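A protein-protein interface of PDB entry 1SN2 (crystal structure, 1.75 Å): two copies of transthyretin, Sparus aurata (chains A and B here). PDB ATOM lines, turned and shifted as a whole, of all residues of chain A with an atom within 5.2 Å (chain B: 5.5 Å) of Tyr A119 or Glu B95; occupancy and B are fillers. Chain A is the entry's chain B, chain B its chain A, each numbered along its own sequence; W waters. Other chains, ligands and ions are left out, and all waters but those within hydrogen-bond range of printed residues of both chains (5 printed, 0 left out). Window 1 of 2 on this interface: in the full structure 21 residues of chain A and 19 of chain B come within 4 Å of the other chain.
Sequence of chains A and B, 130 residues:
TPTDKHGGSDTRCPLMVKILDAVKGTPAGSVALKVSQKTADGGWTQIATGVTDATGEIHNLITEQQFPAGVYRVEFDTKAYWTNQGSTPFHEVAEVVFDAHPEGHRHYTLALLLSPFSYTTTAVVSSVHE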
ATOM      1  N   HIS A  91     -14.757  -7.375 -24.619  1.00  0.00           N
ATOM      2  CA  HIS A  91     -14.424  -7.188 -23.217  1.00  0.00           C
ATOM      3  C   HIS A  91     -13.782  -5.846 -22.903  1.00  0.00           C
ATOM      4  O   HIS A  91     -12.976  -5.310 -23.661  1.00  0.00           O
ATOM      5  CB  HIS A  91     -13.497  -8.307 -22.732  1.00  0.00           C
ATOM      6  CG  HIS A  91     -14.071  -9.686 -22.855  1.00  0.00           C
ATOM      7  ND1 HIS A  91     -13.820 -10.499 -23.939  1.00  0.00           N
ATOM      8  CD2 HIS A  91     -14.810 -10.427 -21.994  1.00  0.00           C
ATOM      9  CE1 HIS A  91     -14.409 -11.668 -23.758  1.00  0.00           C
ATOM     10  NE2 HIS A  91     -15.000 -11.661 -22.578  1.00  0.00           N
ATOM     11  N   VAL A  93     -11.971  -5.433 -20.246  1.00  0.00           N
ATOM     12  CA  VAL A  93     -10.717  -5.812 -19.615  1.00  0.00           C
ATOM     13  C   VAL A  93     -10.755  -7.337 -19.481  1.00  0.00           C
ATOM     14  O   VAL A  93     -11.825  -7.933 -19.566  1.00  0.00           O
ATOM     15  CB  VAL A  93     -10.575  -5.158 -18.215  1.00  0.00           C
ATOM     16  CG1 VAL A  93     -11.688  -5.636 -17.282  1.00  0.00           C
ATOM     17  CG2 VAL A  93      -9.220  -5.454 -17.602  1.00  0.00           C
ATOM     18  N   ALA A  94      -9.599  -7.981 -19.346  1.00  0.00           N
ATOM     19  CA  ALA A  94      -9.559  -9.408 -19.041  1.00  0.00           C
ATOM     20  C   ALA A  94      -8.956  -9.544 -17.642  1.00  0.00           C
ATOM     21  O   ALA A  94      -7.824  -9.105 -17.404  1.00  0.00           O
ATOM     22  CB  ALA A  94      -8.730 -10.164 -20.051  1.00  0.00           C
ATOM     23  N   GLU A  95      -9.717 -10.110 -16.713  1.00  0.00           N
ATOM     24  CA  GLU A  95      -9.244 -10.262 -15.349  1.00  0.00           C
ATOM     25  C   GLU A  95      -9.104 -11.728 -14.997  1.00  0.00           C
ATOM     26  O   GLU A  95     -10.002 -12.537 -15.254  1.00  0.00           O
ATOM     27  CB  GLU A  95     -10.187  -9.612 -14.349  1.00  0.00           C
ATOM     28  CG  GLU A  95     -10.247  -8.096 -14.459  1.00  0.00           C
ATOM     29  CD  GLU A  95     -11.477  -7.515 -13.816  1.00  0.00           C
ATOM     30  OE1 GLU A  95     -12.519  -8.212 -13.748  1.00  0.00           O
ATOM     31  OE2 GLU A  95     -11.411  -6.343 -13.397  1.00  0.00           O
ATOM     32  N   VAL A  97      -8.394 -13.905 -11.690  1.00  0.00           N
ATOM     33  CA  VAL A  97      -8.385 -13.816 -10.237  1.00  0.00           C
ATOM     34  C   VAL A  97      -8.198 -15.216  -9.678  1.00  0.00           C
ATOM     35  O   VAL A  97      -8.970 -16.113  -9.998  1.00  0.00           O
ATOM     36  CB  VAL A  97      -9.691 -13.235  -9.725  1.00  0.00           C
ATOM     37  CG1 VAL A  97      -9.594 -12.977  -8.238  1.00  0.00           C
ATOM     38  CG2 VAL A  97     -10.038 -11.954 -10.480  1.00  0.00           C
ATOM     39  N   LEU A 112      -3.047 -16.712 -21.812  1.00  0.00           N
ATOM     40  CA  LEU A 112      -4.222 -16.010 -22.246  1.00  0.00           C
ATOM     41  C   LEU A 112      -4.299 -16.042 -23.773  1.00  0.00           C
ATOM     42  O   LEU A 112      -3.369 -15.599 -24.427  1.00  0.00           O
ATOM     43  CB  LEU A 112      -4.140 -14.566 -21.738  1.00  0.00           C
ATOM     44  CG  LEU A 112      -5.376 -13.693 -21.757  1.00  0.00           C
ATOM     45  CD1 LEU A 112      -6.467 -14.259 -20.871  1.00  0.00           C
ATOM     46  CD2 LEU A 112      -4.988 -12.294 -21.321  1.00  0.00           C
ATOM     47  N   LEU A 113      -5.404 -16.554 -24.315  1.00  0.00           N
ATOM     48  CA  LEU A 113      -5.602 -16.666 -25.764  1.00  0.00           C
ATOM     49  C   LEU A 113      -6.672 -15.666 -26.175  1.00  0.00           C
ATOM     50  O   LEU A 113      -7.838 -15.831 -25.811  1.00  0.00           O
ATOM     51  CB  LEU A 113      -6.043 -18.081 -26.144  1.00  0.00           C
ATOM     52  CG  LEU A 113      -6.280 -18.279 -27.644  1.00  0.00           C
ATOM     53  CD1 LEU A 113      -5.005 -18.019 -28.405  1.00  0.00           C
ATOM     54  CD2 LEU A 113      -6.814 -19.675 -27.977  1.00  0.00           C
ATOM     55  N   LEU A 114      -6.282 -14.644 -26.938  1.00  0.00           N
ATOM     56  CA  LEU A 114      -7.177 -13.539 -27.266  1.00  0.00           C
ATOM     57  C   LEU A 114      -7.760 -13.526 -28.665  1.00  0.00           C
ATOM     58  O   LEU A 114      -7.039 -13.686 -29.644  1.00  0.00           O
ATOM     59  CB  LEU A 114      -6.429 -12.214 -27.092  1.00  0.00           C
ATOM     60  CG  LEU A 114      -5.755 -11.982 -25.738  1.00  0.00           C
ATOM     61  CD1 LEU A 114      -4.973 -10.667 -25.765  1.00  0.00           C
ATOM     62  CD2 LEU A 114      -6.774 -11.987 -24.609  1.00  0.00           C
ATOM     63  N   SER A 115      -9.074 -13.333 -28.722  1.00  0.00           N
ATOM     64  CA  SER A 115      -9.822 -13.045 -29.947  1.00  0.00           C
ATOM     65  C   SER A 115     -10.694 -11.819 -29.589  1.00  0.00           C
ATOM     66  O   SER A 115     -10.988 -11.580 -28.413  1.00  0.00           O
ATOM     67  CB  SER A 115     -10.714 -14.198 -30.378  1.00  0.00           C
ATOM     68  OG  SER A 115      -9.985 -15.397 -30.629  1.00  0.00           O
ATOM     69  N   PHE A 117     -13.867 -11.188 -29.590  1.00  0.00           N
ATOM     70  CA  PHE A 117     -15.072 -11.485 -28.827  1.00  0.00           C
ATOM     71  C   PHE A 117     -14.951 -12.717 -27.924  1.00  0.00           C
ATOM     72  O   PHE A 117     -15.953 -13.255 -27.461  1.00  0.00           O
ATOM     73  CB  PHE A 117     -16.298 -11.554 -29.745  1.00  0.00           C
ATOM     74  CG  PHE A 117     -17.036 -10.252 -29.805  1.00  0.00           C
ATOM     75  CD1 PHE A 117     -16.399  -9.123 -30.286  1.00  0.00           C
ATOM     76  CD2 PHE A 117     -18.319 -10.131 -29.311  1.00  0.00           C
ATOM     77  CE1 PHE A 117     -17.040  -7.898 -30.297  1.00  0.00           C
ATOM     78  CE2 PHE A 117     -18.971  -8.900 -29.333  1.00  0.00           C
ATOM     79  CZ  PHE A 117     -18.327  -7.795 -29.822  1.00  0.00           C
ATOM     80  N   SER A 118     -13.720 -13.131 -27.631  1.00  0.00           N
ATOM     81  CA  SER A 118     -13.509 -14.305 -26.787  1.00  0.00           C
ATOM     82  C   SER A 118     -12.093 -14.376 -26.240  1.00  0.00           C
ATOM     83  O   SER A 118     -11.142 -13.958 -26.885  1.00  0.00           O
ATOM     84  CB  SER A 118     -13.787 -15.574 -27.620  1.00  0.00           C
ATOM     85  OG  SER A 118     -13.730 -16.751 -26.834  1.00  0.00           O
ATOM     86  N   TYR A 119     -11.944 -14.865 -25.019  1.00  0.00           N
ATOM     87  CA  TYR A 119     -10.607 -15.196 -24.561  1.00  0.00           C
ATOM     88  C   TYR A 119     -10.653 -16.412 -23.685  1.00  0.00           C
ATOM     89  O   TYR A 119     -11.678 -16.725 -23.074  1.00  0.00           O
ATOM     90  CB  TYR A 119      -9.862 -14.042 -23.891  1.00  0.00           C
ATOM     91  CG  TYR A 119     -10.428 -13.497 -22.595  1.00  0.00           C
ATOM     92  CD1 TYR A 119     -10.210 -14.148 -21.387  1.00  0.00           C
ATOM     93  CD2 TYR A 119     -11.118 -12.302 -22.577  1.00  0.00           C
ATOM     94  CE1 TYR A 119     -10.707 -13.635 -20.203  1.00  0.00           C
ATOM     95  CE2 TYR A 119     -11.604 -11.781 -21.406  1.00  0.00           C
ATOM     96  CZ  TYR A 119     -11.400 -12.450 -20.221  1.00  0.00           C
ATOM     97  OH  TYR A 119     -11.884 -11.925 -19.052  1.00  0.00           O
ATOM     98  N   THR A 120      -9.518 -17.088 -23.643  1.00  0.00           N
ATOM     99  CA  THR A 120      -9.328 -18.276 -22.831  1.00  0.00           C
ATOM    100  C   THR A 120      -8.230 -17.979 -21.844  1.00  0.00           C
ATOM    101  O   THR A 120      -7.149 -17.530 -22.223  1.00  0.00           O
ATOM    102  CB  THR A 120      -8.942 -19.476 -23.705  1.00  0.00           C
ATOM    103  OG1 THR A 120     -10.034 -19.814 -24.564  1.00  0.00           O
ATOM    104  CG2 THR A 120      -8.739 -20.706 -22.854  1.00  0.00           C
ATOM    105  N   THR A 121      -8.546 -18.179 -20.567  1.00  0.00           N
ATOM    106  CA  THR A 121      -7.593 -18.003 -19.489  1.00  0.00           C
ATOM    107  C   THR A 121      -7.334 -19.368 -18.858  1.00  0.00           C
ATOM    108  O   THR A 121      -8.258 -20.041 -18.378  1.00  0.00           O
ATOM    109  CB  THR A 121      -8.110 -16.993 -18.442  1.00  0.00           C
ATOM    110  OG1 THR A 121      -7.466 -17.205 -17.168  1.00  0.00           O
ATOM    111  CG2 THR A 121      -9.587 -17.192 -18.146  1.00  0.00           C
ATOM    112  N   ARG B  73     -20.393  -6.049 -15.157  1.00  0.00           N
ATOM    113  CA  ARG B  73     -19.531  -7.125 -14.728  1.00  0.00           C
ATOM    114  C   ARG B  73     -20.414  -8.288 -14.321  1.00  0.00           C
ATOM    115  O   ARG B  73     -21.324  -8.126 -13.515  1.00  0.00           O
ATOM    116  CB  ARG B  73     -18.722  -6.695 -13.518  1.00  0.00           C
ATOM    117  CG  ARG B  73     -17.615  -7.626 -13.178  1.00  0.00           C
ATOM    118  CD  ARG B  73     -17.862  -8.474 -11.961  1.00  0.00           C
ATOM    119  NE  ARG B  73     -17.952  -7.720 -10.707  1.00  0.00           N
ATOM    120  CZ  ARG B  73     -17.110  -6.774 -10.318  1.00  0.00           C
ATOM    121  NH1 ARG B  73     -16.087  -6.411 -11.086  1.00  0.00           N
ATOM    122  NH2 ARG B  73     -17.295  -6.178  -9.142  1.00  0.00           N
ATOM    123  N   VAL B  74     -20.160  -9.454 -14.895  1.00  0.00           N
ATOM    124  CA  VAL B  74     -20.888 -10.641 -14.518  1.00  0.00           C
ATOM    125  C   VAL B  74     -19.843 -11.530 -13.875  1.00  0.00           C
ATOM    126  O   VAL B  74     -18.834 -11.863 -14.498  1.00  0.00           O
ATOM    127  CB  VAL B  74     -21.558 -11.351 -15.709  1.00  0.00           C
ATOM    128  CG1 VAL B  74     -22.362 -12.529 -15.220  1.00  0.00           C
ATOM    129  CG2 VAL B  74     -22.458 -10.397 -16.478  1.00  0.00           C
ATOM    130  N   GLU B  75     -20.097 -11.890 -12.624  1.00  0.00           N
ATOM    131  CA  GLU B  75     -19.187 -12.697 -11.828  1.00  0.00           C
ATOM    132  C   GLU B  75     -19.809 -14.055 -11.578  1.00  0.00           C
ATOM    133  O   GLU B  75     -20.912 -14.144 -11.030  1.00  0.00           O
ATOM    134  CB  GLU B  75     -18.928 -11.986 -10.501  1.00  0.00           C
ATOM    135  CG  GLU B  75     -17.892 -12.671  -9.627  1.00  0.00           C
ATOM    136  CD  GLU B  75     -17.416 -11.801  -8.477  1.00  0.00           C
ATOM    137  OE1 GLU B  75     -16.928 -10.669  -8.741  1.00  0.00           O
ATOM    138  OE2 GLU B  75     -17.535 -12.251  -7.311  1.00  0.00           O
ATOM    139  N   PHE B  76     -19.086 -15.110 -11.955  1.00  0.00           N
ATOM    140  CA  PHE B  76     -19.557 -16.473 -11.838  1.00  0.00           C
ATOM    141  C   PHE B  76     -18.759 -17.187 -10.748  1.00  0.00           C
ATOM    142  O   PHE B  76     -17.523 -17.146 -10.765  1.00  0.00           O
ATOM    143  CB  PHE B  76     -19.335 -17.238 -13.154  1.00  0.00           C
ATOM    144  CG  PHE B  76     -20.010 -16.633 -14.359  1.00  0.00           C
ATOM    145  CD1 PHE B  76     -19.419 -15.596 -15.064  1.00  0.00           C
ATOM    146  CD2 PHE B  76     -21.203 -17.144 -14.820  1.00  0.00           C
ATOM    147  CE1 PHE B  76     -20.032 -15.067 -16.187  1.00  0.00           C
ATOM    148  CE2 PHE B  76     -21.811 -16.626 -15.935  1.00  0.00           C
ATOM    149  CZ  PHE B  76     -21.221 -15.580 -16.621  1.00  0.00           C
ATOM    150  N   VAL B  93     -12.866 -16.856  -9.163  1.00  0.00           N
ATOM    151  CA  VAL B  93     -14.123 -16.496  -9.770  1.00  0.00           C
ATOM    152  C   VAL B  93     -13.860 -16.330 -11.258  1.00  0.00           C
ATOM    153  O   VAL B  93     -12.704 -16.178 -11.664  1.00  0.00           O
ATOM    154  CB  VAL B  93     -14.610 -15.144  -9.192  1.00  0.00           C
ATOM    155  CG1 VAL B  93     -13.576 -14.059  -9.413  1.00  0.00           C
ATOM    156  CG2 VAL B  93     -15.929 -14.762  -9.865  1.00  0.00           C
ATOM    157  N   ALA B  94     -14.902 -16.409 -12.080  1.00  0.00           N
ATOM    158  CA  ALA B  94     -14.755 -16.074 -13.487  1.00  0.00           C
ATOM    159  C   ALA B  94     -15.447 -14.730 -13.676  1.00  0.00           C
ATOM    160  O   ALA B  94     -16.617 -14.578 -13.327  1.00  0.00           O
ATOM    161  CB  ALA B  94     -15.367 -17.109 -14.359  1.00  0.00           C
ATOM    162  N   GLU B  95     -14.732 -13.758 -14.218  1.00  0.00           N
ATOM    163  CA  GLU B  95     -15.300 -12.428 -14.369  1.00  0.00           C
ATOM    164  C   GLU B  95     -15.393 -12.007 -15.824  1.00  0.00           C
ATOM    165  O   GLU B  95     -14.448 -12.186 -16.603  1.00  0.00           O
ATOM    166  CB  GLU B  95     -14.520 -11.416 -13.535  1.00  0.00           C
ATOM    167  CG  GLU B  95     -15.324 -10.983 -12.309  1.00  0.00           C
ATOM    168  CD  GLU B  95     -14.483 -10.474 -11.178  1.00  0.00           C
ATOM    169  OE1 GLU B  95     -14.693 -10.973 -10.052  1.00  0.00           O
ATOM    170  OE2 GLU B  95     -13.638  -9.570 -11.406  1.00  0.00           O
ATOM    171  N   VAL B  96     -16.552 -11.475 -16.197  1.00  0.00           N
ATOM    172  CA  VAL B  96     -16.778 -11.019 -17.564  1.00  0.00           C
ATOM    173  C   VAL B  96     -17.221  -9.566 -17.471  1.00  0.00           C
ATOM    174  O   VAL B  96     -18.319  -9.280 -16.977  1.00  0.00           O
ATOM    175  CB  VAL B  96     -17.834 -11.872 -18.295  1.00  0.00           C
ATOM    176  CG1 VAL B  96     -18.067 -11.357 -19.703  1.00  0.00           C
ATOM    177  CG2 VAL B  96     -17.403 -13.322 -18.364  1.00  0.00           C
ATOM    178  N   VAL B  97     -16.367  -8.669 -17.946  1.00  0.00           N
ATOM    179  CA  VAL B  97     -16.562  -7.223 -17.826  1.00  0.00           C
ATOM    180  C   VAL B  97     -16.634  -6.647 -19.219  1.00  0.00           C
ATOM    181  O   VAL B  97     -15.699  -6.842 -20.013  1.00  0.00           O
ATOM    182  CB  VAL B  97     -15.380  -6.555 -17.105  1.00  0.00           C
ATOM    183  CG1 VAL B  97     -15.696  -5.076 -16.798  1.00  0.00           C
ATOM    184  CG2 VAL B  97     -15.039  -7.311 -15.838  1.00  0.00           C
ATOM    185  N   TYR B 119     -10.903 -21.360 -18.287  1.00  0.00           N
ATOM    186  CA  TYR B 119     -12.223 -21.027 -18.807  1.00  0.00           C
ATOM    187  C   TYR B 119     -12.134 -20.148 -20.045  1.00  0.00           C
ATOM    188  O   TYR B 119     -11.151 -19.418 -20.241  1.00  0.00           O
ATOM    189  CB  TYR B 119     -13.156 -20.448 -17.745  1.00  0.00           C
ATOM    190  CG  TYR B 119     -12.854 -19.084 -17.179  1.00  0.00           C
ATOM    191  CD1 TYR B 119     -13.167 -17.933 -17.872  1.00  0.00           C
ATOM    192  CD2 TYR B 119     -12.314 -18.956 -15.910  1.00  0.00           C
ATOM    193  CE1 TYR B 119     -12.926 -16.676 -17.310  1.00  0.00           C
ATOM    194  CE2 TYR B 119     -12.076 -17.722 -15.352  1.00  0.00           C
ATOM    195  CZ  TYR B 119     -12.376 -16.589 -16.050  1.00  0.00           C
ATOM    196  OH  TYR B 119     -12.119 -15.364 -15.476  1.00  0.00           O
ATOM    197  N   THR B 120     -13.148 -20.274 -20.890  1.00  0.00           N
ATOM    198  CA  THR B 120     -13.259 -19.487 -22.109  1.00  0.00           C
ATOM    199  C   THR B 120     -14.529 -18.665 -21.998  1.00  0.00           C
ATOM    200  O   THR B 120     -15.608 -19.214 -21.764  1.00  0.00           O
ATOM    201  CB  THR B 120     -13.318 -20.415 -23.338  1.00  0.00           C
ATOM    202  OG1 THR B 120     -12.082 -21.134 -23.478  1.00  0.00           O
ATOM    203  CG2 THR B 120     -13.459 -19.623 -24.633  1.00  0.00           C
ATOM    204  N   THR B 121     -14.383 -17.343 -22.120  1.00  0.00           N
ATOM    205  CA  THR B 121     -15.507 -16.410 -22.115  1.00  0.00           C
ATOM    206  C   THR B 121     -15.670 -15.851 -23.524  1.00  0.00           C
ATOM    207  O   THR B 121     -14.742 -15.268 -24.081  1.00  0.00           O
ATOM    208  CB  THR B 121     -15.341 -15.257 -21.081  1.00  0.00           C
ATOM    209  OG1 THR B 121     -16.136 -14.119 -21.472  1.00  0.00           O
ATOM    210  CG2 THR B 121     -13.929 -14.714 -21.021  1.00  0.00           C
ATOM    211  N   THR B 122     -16.846 -16.064 -24.098  1.00  0.00           N
ATOM    212  CA  THR B 122     -17.174 -15.585 -25.421  1.00  0.00           C
ATOM    213  C   THR B 122     -18.475 -14.826 -25.304  1.00  0.00           C
ATOM    214  O   THR B 122     -19.297 -15.108 -24.427  1.00  0.00           O
ATOM    215  CB  THR B 122     -17.400 -16.782 -26.371  1.00  0.00           C
ATOM    216  OG1 THR B 122     -16.251 -17.641 -26.371  1.00  0.00           O
ATOM    217  CG2 THR B 122     -17.563 -16.316 -27.810  1.00  0.00           C
HETATM  218  O   HOH W   1     -12.023 -13.117 -16.811  1.00  0.00           O
HETATM  219  O   HOH W   2     -13.772  -9.782 -18.798  1.00  0.00           O
HETATM  220  O   HOH W   3     -13.952  -5.441 -12.678  1.00  0.00           O
HETATM  221  O   HOH W   4     -10.685 -15.040 -13.055  1.00  0.00           O
HETATM  222  O   HOH W   5     -12.521  -9.872 -16.320  1.00  0.00           O
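Of chain B, only Glu B95, Tyr B119, Thr B120 and Thr B121 come within 4 Å of Tyr A119. Glu B95 touches two residues of chain A. Printed residues of chain B within 4 Å of His A91: Val B97 (3.5 Å) and Thr B121 (2.9 Å). Of the printed residues of chain A, Val B97 touches His A91 (3.5 Å), Val A93 (3.8 Å) and Glu A95 (3.4 Å). Ser A115 touches none of the printed residues of chain B. The nearest residue of chain B that does not touch Tyr A119 is Thr B122 (5.1 Å). The nearest residue of chain A that does not touch Glu B95 is Val A97 (4.4 Å). The nearest printed residue of chain A that does not touch Val B93 is Glu A95 (5.8 Å).
The backbone NH of Thr B121 sits at hydrogen-bond distance from the backbone carbonyl oxygen of Tyr A119, at 2.9 Å. OE1 of Glu A95 lies close to OE2 of Glu B95, at 2.9 Å. The side-chain hydroxyl (OG1) of Thr B121 sits at hydrogen-bond distance from a ring nitrogen (NE2) of His A91. OG1 of Thr B122 lies within hydrogen-bond range of OG of Ser A118 (2.7 Å). O of Thr B121 sits close to OG of Ser A118 (3.3 Å). The backbone NH of Thr A121 is in hydrogen-bond range of the backbone carbonyl oxygen of Tyr B119 (2.9 Å). The side-chain hydroxyl (OG1) of Thr B120 sits at hydrogen-bond distance from the side-chain hydroxyl (OG1) of Thr A120 (2.7 Å).
Water W1 lies within hydrogen-bond range of OH of Tyr A119, O of Glu B95, OH of Tyr B119 and O of Glu A95. Water W4 lies within hydrogen-bond range of O of Val B93, OH of Tyr B119, N of Val A97 and O of Glu A95. Water W3 lies within hydrogen-bond range of the side-chain carboxylate (OE2) of Glu A95 (2.8 Å) and the guanidinium group (NH1) of Arg B73 (2.8 Å). Water W2 lies within hydrogen-bond range of O of Val A93 (2.8 Å), OH of Tyr A119 (2.9 Å), N of Val B97 (2.9 Å) and O of Glu B95 (3.3 Å). Water W5 lies within hydrogen-bond range of the backbone NH of Glu A95 (2.8 Å), the backbone carbonyl oxygen of Glu B95 (3.0 Å) and the side-chain hydroxyl of Tyr A119 (3.5 Å).
Among the printed residues, pairs that only touch across the chains: Tyr A119 with Thr B120 (3.3 Å), Phe A117 with Thr B122 (3.3 Å), Thr A120 with Tyr B119 (3.4 Å), Glu A95 with Val B97 (3.4 Å), His A91 with Val B97 (3.5 Å), Glu A95 with Tyr B119 (3.5 Å), Tyr A119 with Glu B95 (3.6 Å), Ser A118 with Thr B120 (3.6 Å), Val A93 with Val B97 (3.8 Å), Tyr A119 with Tyr B119 (3.9 Å) and Val A97 with Val B93 (3.98 Å).
N of Glu B95 lies within hydrogen-bond range of OH of Tyr B119 (3.3 Å). The side-chain carboxylate of Glu B75 lies close to the side-chain carboxylate of Glu B95 (2.6 Å). The backbone NH (N) of Leu A113 lies within hydrogen-bond range of the backbone carbonyl oxygen (O) of Thr A120.
Hydrophobic or aromatic side chains of chain A that line the printed part of chain B: His A91, Val A93, Val A97 and Tyr A119. Along chain A the printed residues that touch a printed residue of chain B span positions 91 to 121. Of the 13 printed residues of chain B, 7 touch a printed residue of chain A. Among the printed residues, 18 pairs touch across the chains. Among the printed residues, no Asp or Glu carboxylate lies within 4 Å of a Lys or Arg side-chain nitrogen of the other chain.
Glu A95 touches Tyr B119, and with the chains exchanged Tyr A119 touches Glu B95. Tyr A119 touches its own counterpart, Tyr B119. Tyr A119 touches Thr B120, and with the chains exchanged Thr A120 touches Tyr B119. Thr A120 touches its own counterpart, Thr B120. Positions printed for both chains: 93, 94, 95, 97, 119, 120 and 121. Of the 18 pairs that touch across the chains among the printed residues, 11 have their exchanged pair printed and touching as well.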
